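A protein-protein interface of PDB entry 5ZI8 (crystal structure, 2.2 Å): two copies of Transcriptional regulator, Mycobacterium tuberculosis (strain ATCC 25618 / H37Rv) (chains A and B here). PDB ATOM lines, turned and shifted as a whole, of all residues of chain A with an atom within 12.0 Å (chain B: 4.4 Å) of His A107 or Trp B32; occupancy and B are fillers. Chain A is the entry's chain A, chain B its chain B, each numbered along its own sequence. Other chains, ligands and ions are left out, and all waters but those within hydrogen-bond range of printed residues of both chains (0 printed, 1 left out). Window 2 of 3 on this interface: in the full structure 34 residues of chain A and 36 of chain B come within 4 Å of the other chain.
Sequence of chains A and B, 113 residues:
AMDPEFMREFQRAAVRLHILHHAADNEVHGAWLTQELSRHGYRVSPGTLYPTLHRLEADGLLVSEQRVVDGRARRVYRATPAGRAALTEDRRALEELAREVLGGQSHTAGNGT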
ATOM      1  N   ARG A  99      -2.711  -9.234   0.250  1.00  0.00           N
ATOM      2  CA  ARG A  99      -3.267  -7.859   0.402  1.00  0.00           C
ATOM      3  C   ARG A  99      -4.653  -7.653  -0.179  1.00  0.00           C
ATOM      4  O   ARG A  99      -5.435  -6.996   0.405  1.00  0.00           O
ATOM      5  CB  ARG A  99      -2.374  -6.777  -0.248  1.00  0.00           C
ATOM      6  CG  ARG A  99      -1.092  -6.375   0.434  1.00  0.00           C
ATOM      7  CD  ARG A  99      -0.662  -5.049  -0.146  1.00  0.00           C
ATOM      8  NE  ARG A  99      -0.346  -5.122  -1.573  1.00  0.00           N
ATOM      9  CZ  ARG A  99       0.801  -5.584  -2.113  1.00  0.00           C
ATOM     10  NH1 ARG A  99       1.804  -6.062  -1.357  1.00  0.00           N
ATOM     11  NH2 ARG A  99       0.946  -5.566  -3.448  1.00  0.00           N
ATOM     12  N   GLU A 100      -4.911  -8.166  -1.373  1.00  0.00           N
ATOM     13  CA  GLU A 100      -6.208  -8.044  -2.056  1.00  0.00           C
ATOM     14  C   GLU A 100      -7.401  -8.729  -1.346  1.00  0.00           C
ATOM     15  O   GLU A 100      -8.496  -8.137  -1.223  1.00  0.00           O
ATOM     16  CB  GLU A 100      -6.106  -8.624  -3.468  1.00  0.00           C
ATOM     17  CG  GLU A 100      -5.256  -7.781  -4.445  1.00  0.00           C
ATOM     18  CD  GLU A 100      -4.788  -8.498  -5.689  1.00  0.00           C
ATOM     19  OE1 GLU A 100      -4.788  -9.753  -5.813  1.00  0.00           O
ATOM     20  OE2 GLU A 100      -4.334  -7.726  -6.560  1.00  0.00           O
ATOM     21  N   VAL A 101      -7.184  -9.961  -0.890  1.00  0.00           N
ATOM     22  CA  VAL A 101      -8.270 -10.859  -0.523  1.00  0.00           C
ATOM     23  C   VAL A 101      -8.503 -10.967   0.960  1.00  0.00           C
ATOM     24  O   VAL A 101      -9.535 -11.503   1.386  1.00  0.00           O
ATOM     25  CB  VAL A 101      -8.061 -12.209  -1.283  1.00  0.00           C
ATOM     26  CG1 VAL A 101      -8.087 -13.449  -0.395  1.00  0.00           C
ATOM     27  CG2 VAL A 101      -9.030 -12.223  -2.453  1.00  0.00           C
ATOM     28  N   LEU A 102      -7.543 -10.496   1.728  1.00  0.00           N
ATOM     29  CA  LEU A 102      -7.698 -10.350   3.166  1.00  0.00           C
ATOM     30  C   LEU A 102      -8.014  -8.887   3.622  1.00  0.00           C
ATOM     31  O   LEU A 102      -7.665  -8.505   4.674  1.00  0.00           O
ATOM     32  CB  LEU A 102      -6.465 -10.957   3.870  1.00  0.00           C
ATOM     33  CG  LEU A 102      -5.903 -12.301   3.264  1.00  0.00           C
ATOM     34  CD1 LEU A 102      -4.597 -12.785   3.859  1.00  0.00           C
ATOM     35  CD2 LEU A 102      -6.869 -13.469   3.342  1.00  0.00           C
ATOM     36  N   GLY A 103      -8.733  -8.068   2.852  1.00  0.00           N
ATOM     37  CA  GLY A 103      -9.304  -6.780   3.389  1.00  0.00           C
ATOM     38  C   GLY A 103     -10.410  -6.190   2.517  1.00  0.00           C
ATOM     39  O   GLY A 103     -10.675  -4.974   2.569  1.00  0.00           O
ATOM     40  N   HIS A 107     -16.338  -3.052  -2.563  1.00  0.00           N
ATOM     41  CA  HIS A 107     -17.553  -3.166  -3.363  1.00  0.00           C
ATOM     42  C   HIS A 107     -18.748  -3.366  -2.430  1.00  0.00           C
ATOM     43  O   HIS A 107     -19.535  -2.449  -2.233  1.00  0.00           O
ATOM     44  CB  HIS A 107     -17.493  -4.341  -4.391  1.00  0.00           C
ATOM     45  CG  HIS A 107     -16.191  -4.473  -5.129  1.00  0.00           C
ATOM     46  ND1 HIS A 107     -15.863  -3.665  -6.199  1.00  0.00           N
ATOM     47  CD2 HIS A 107     -15.144  -5.320  -4.962  1.00  0.00           C
ATOM     48  CE1 HIS A 107     -14.666  -3.994  -6.652  1.00  0.00           C
ATOM     49  NE2 HIS A 107     -14.211  -4.998  -5.924  1.00  0.00           N
ATOM     50  N   HIS B  22     -15.270 -11.741  -4.852  1.00  0.00           N
ATOM     51  CA  HIS B  22     -16.189 -10.777  -5.437  1.00  0.00           C
ATOM     52  C   HIS B  22     -17.671 -11.190  -5.388  1.00  0.00           C
ATOM     53  O   HIS B  22     -18.520 -10.347  -5.139  1.00  0.00           O
ATOM     54  CB  HIS B  22     -15.764 -10.448  -6.863  1.00  0.00           C
ATOM     55  CG  HIS B  22     -14.598  -9.540  -6.897  1.00  0.00           C
ATOM     56  ND1 HIS B  22     -13.298  -9.998  -6.791  1.00  0.00           N
ATOM     57  CD2 HIS B  22     -14.536  -8.192  -6.935  1.00  0.00           C
ATOM     58  CE1 HIS B  22     -12.483  -8.960  -6.822  1.00  0.00           C
ATOM     59  NE2 HIS B  22     -13.213  -7.858  -6.918  1.00  0.00           N
ATOM     60  N   ASP B  25     -19.376 -10.615  -1.890  1.00  0.00           N
ATOM     61  CA  ASP B  25     -19.743  -9.193  -1.706  1.00  0.00           C
ATOM     62  C   ASP B  25     -21.107  -8.791  -2.384  1.00  0.00           C
ATOM     63  O   ASP B  25     -21.910  -8.052  -1.776  1.00  0.00           O
ATOM     64  CB  ASP B  25     -18.530  -8.363  -2.286  1.00  0.00           C
ATOM     65  CG  ASP B  25     -18.381  -6.949  -1.738  1.00  0.00           C
ATOM     66  OD1 ASP B  25     -19.328  -6.353  -1.135  1.00  0.00           O
ATOM     67  OD2 ASP B  25     -17.253  -6.417  -1.979  1.00  0.00           O
ATOM     68  N   VAL B  28     -22.616 -10.553  -9.575  1.00  0.00           N
ATOM     69  CA  VAL B  28     -21.696 -10.142 -10.606  1.00  0.00           C
ATOM     70  C   VAL B  28     -22.033 -10.816 -11.946  1.00  0.00           C
ATOM     71  O   VAL B  28     -22.485 -11.947 -11.999  1.00  0.00           O
ATOM     72  CB  VAL B  28     -20.223 -10.476 -10.197  1.00  0.00           C
ATOM     73  CG1 VAL B  28     -19.872  -9.897  -8.840  1.00  0.00           C
ATOM     74  CG2 VAL B  28     -19.952 -11.961 -10.162  1.00  0.00           C
ATOM     75  N   HIS B  29     -21.835 -10.077 -13.032  1.00  0.00           N
ATOM     76  CA  HIS B  29     -21.869 -10.590 -14.388  1.00  0.00           C
ATOM     77  C   HIS B  29     -20.442 -10.973 -14.713  1.00  0.00           C
ATOM     78  O   HIS B  29     -19.482 -10.414 -14.149  1.00  0.00           O
ATOM     79  CB  HIS B  29     -22.321  -9.495 -15.357  1.00  0.00           C
ATOM     80  CG  HIS B  29     -23.710  -9.004 -15.114  1.00  0.00           C
ATOM     81  ND1 HIS B  29     -23.966  -7.763 -14.575  1.00  0.00           N
ATOM     82  CD2 HIS B  29     -24.914  -9.582 -15.353  1.00  0.00           C
ATOM     83  CE1 HIS B  29     -25.285  -7.611 -14.466  1.00  0.00           C
ATOM     84  NE2 HIS B  29     -25.879  -8.704 -14.934  1.00  0.00           N
ATOM     85  N   GLY B  30     -20.294 -11.904 -15.645  1.00  0.00           N
ATOM     86  CA  GLY B  30     -19.001 -12.301 -16.070  1.00  0.00           C
ATOM     87  C   GLY B  30     -18.282 -11.216 -16.835  1.00  0.00           C
ATOM     88  O   GLY B  30     -17.053 -11.099 -16.741  1.00  0.00           O
ATOM     89  N   ALA B  31     -19.012 -10.400 -17.577  1.00  0.00           N
ATOM     90  CA  ALA B  31     -18.362  -9.319 -18.300  1.00  0.00           C
ATOM     91  C   ALA B  31     -17.648  -8.430 -17.319  1.00  0.00           C
ATOM     92  O   ALA B  31     -16.450  -8.128 -17.461  1.00  0.00           O
ATOM     93  CB  ALA B  31     -19.383  -8.532 -19.086  1.00  0.00           C
ATOM     94  N   TRP B  32     -18.359  -8.078 -16.256  1.00  0.00           N
ATOM     95  CA  TRP B  32     -17.767  -7.228 -15.227  1.00  0.00           C
ATOM     96  C   TRP B  32     -16.592  -7.891 -14.525  1.00  0.00           C
ATOM     97  O   TRP B  32     -15.600  -7.213 -14.234  1.00  0.00           O
ATOM     98  CB  TRP B  32     -18.755  -6.818 -14.195  1.00  0.00           C
ATOM     99  CG  TRP B  32     -18.227  -5.852 -13.219  1.00  0.00           C
ATOM    100  CD1 TRP B  32     -18.106  -4.526 -13.412  1.00  0.00           C
ATOM    101  CD2 TRP B  32     -17.807  -6.087 -11.880  1.00  0.00           C
ATOM    102  NE1 TRP B  32     -17.639  -3.889 -12.288  1.00  0.00           N
ATOM    103  CE2 TRP B  32     -17.449  -4.822 -11.320  1.00  0.00           C
ATOM    104  CE3 TRP B  32     -17.749  -7.206 -11.080  1.00  0.00           C
ATOM    105  CZ2 TRP B  32     -16.969  -4.667 -10.019  1.00  0.00           C
ATOM    106  CZ3 TRP B  32     -17.314  -7.061  -9.758  1.00  0.00           C
ATOM    107  CH2 TRP B  32     -16.922  -5.790  -9.237  1.00  0.00           C
ATOM    108  N   LEU B  33     -16.715  -9.181 -14.217  1.00  0.00           N
ATOM    109  CA  LEU B  33     -15.621  -9.865 -13.556  1.00  0.00           C
ATOM    110  C   LEU B  33     -14.323  -9.844 -14.356  1.00  0.00           C
ATOM    111  O   LEU B  33     -13.254  -9.789 -13.782  1.00  0.00           O
ATOM    112  CB  LEU B  33     -15.941 -11.322 -13.307  1.00  0.00           C
ATOM    113  CG  LEU B  33     -16.567 -11.662 -11.978  1.00  0.00           C
ATOM    114  CD1 LEU B  33     -16.709 -13.154 -11.927  1.00  0.00           C
ATOM    115  CD2 LEU B  33     -15.785 -11.143 -10.774  1.00  0.00           C
ATOM    116  N   THR B  34     -14.425  -9.943 -15.674  1.00  0.00           N
ATOM    117  CA  THR B  34     -13.261  -9.851 -16.535  1.00  0.00           C
ATOM    118  C   THR B  34     -12.554  -8.517 -16.309  1.00  0.00           C
ATOM    119  O   THR B  34     -11.344  -8.482 -16.100  1.00  0.00           O
ATOM    120  CB  THR B  34     -13.666 -10.056 -18.015  1.00  0.00           C
ATOM    121  OG1 THR B  34     -14.402 -11.289 -18.151  1.00  0.00           O
ATOM    122  CG2 THR B  34     -12.472 -10.211 -18.863  1.00  0.00           C
ATOM    123  N   GLN B  35     -13.328  -7.438 -16.280  1.00  0.00           N
ATOM    124  CA  GLN B  35     -12.773  -6.086 -16.103  1.00  0.00           C
ATOM    125  C   GLN B  35     -12.119  -5.931 -14.717  1.00  0.00           C
ATOM    126  O   GLN B  35     -11.009  -5.417 -14.565  1.00  0.00           O
ATOM    127  CB  GLN B  35     -13.851  -4.995 -16.313  1.00  0.00           C
ATOM    128  CG  GLN B  35     -14.637  -5.053 -17.638  1.00  0.00           C
ATOM    129  CD  GLN B  35     -13.808  -4.742 -18.887  1.00  0.00           C
ATOM    130  OE1 GLN B  35     -12.667  -5.169 -19.063  1.00  0.00           O
ATOM    131  NE2 GLN B  35     -14.385  -3.952 -19.750  1.00  0.00           N
ATOM    132  N   GLU B  36     -12.812  -6.410 -13.708  1.00  0.00           N
ATOM    133  CA  GLU B  36     -12.366  -6.262 -12.349  1.00  0.00           C
ATOM    134  C   GLU B  36     -11.113  -7.081 -12.041  1.00  0.00           C
ATOM    135  O   GLU B  36     -10.228  -6.606 -11.349  1.00  0.00           O
ATOM    136  CB  GLU B  36     -13.522  -6.622 -11.426  1.00  0.00           C
ATOM    137  CG  GLU B  36     -13.265  -6.411  -9.964  1.00  0.00           C
ATOM    138  CD  GLU B  36     -13.041  -4.976  -9.542  1.00  0.00           C
ATOM    139  OE1 GLU B  36     -13.414  -4.053 -10.250  1.00  0.00           O
ATOM    140  OE2 GLU B  36     -12.530  -4.819  -8.434  1.00  0.00           O
ATOM    141  N   ARG B  39      -8.399  -5.253 -13.618  1.00  0.00           N
ATOM    142  CA  ARG B  39      -7.929  -4.206 -12.695  1.00  0.00           C
ATOM    143  C   ARG B  39      -6.996  -4.791 -11.641  1.00  0.00           C
ATOM    144  O   ARG B  39      -5.999  -4.196 -11.355  1.00  0.00           O
ATOM    145  CB  ARG B  39      -9.046  -3.496 -11.944  1.00  0.00           C
ATOM    146  CG  ARG B  39      -9.840  -2.479 -12.737  1.00  0.00           C
ATOM    147  CD  ARG B  39     -11.144  -2.062 -12.027  1.00  0.00           C
ATOM    148  NE  ARG B  39     -12.164  -1.765 -13.024  1.00  0.00           N
ATOM    149  CZ  ARG B  39     -13.360  -2.346 -13.151  1.00  0.00           C
ATOM    150  NH1 ARG B  39     -13.820  -3.259 -12.332  1.00  0.00           N
ATOM    151  NH2 ARG B  39     -14.153  -1.962 -14.132  1.00  0.00           N
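A ring nitrogen (NE2) of His A107 lies close to a ring nitrogen (NE2) of His B22, 3.2 Å away. The side-chain carboxylate of Glu B36 lies close to a ring nitrogen (NE2) of His A107 (3.0 Å).
The side-chain carboxylate (OE1) of Glu B36 is in salt-bridge range of the guanidinium group (NE) of Arg B39.
Among the printed residues, merely in contact across the chains: His A107 with Asp B25 and His A107 with Trp B32.
Of the printed residues of chain B, His A107 touches His B22 (3.2 Å), Asp B25 (3.2 Å), Trp B32 (3.9 Å) and Glu B36 (2.9 Å). Of chain A, only His A107 comes within 4 Å of His B22. Val B28 touches none of the printed residues of chain A. No residue of chain A comes within 4 Å of His B29. No residue of chain A comes within 4 Å of Ala B31. Of chain A, only His A107 (3.9 Å) comes within 4 Å of Trp B32. No residue of chain A comes within 4 Å of Gln B35. Glu B36 touches one residue of chain A. The nearest printed residue of chain B that does not touch His A107 is Arg B39 (5.8 Å).
Of the 6 printed residues of chain A, 1 touches a printed residue of chain B. Hydrophobic or aromatic side chains of chain A that line the printed part of chain B: His A107. Among the printed residues, 4 pairs touch across the chains. Among the printed residues, no Asp or Glu carboxylate lies within 4 Å of a Lys or Arg side-chain nitrogen of the other chain.
No position is printed for both chains.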
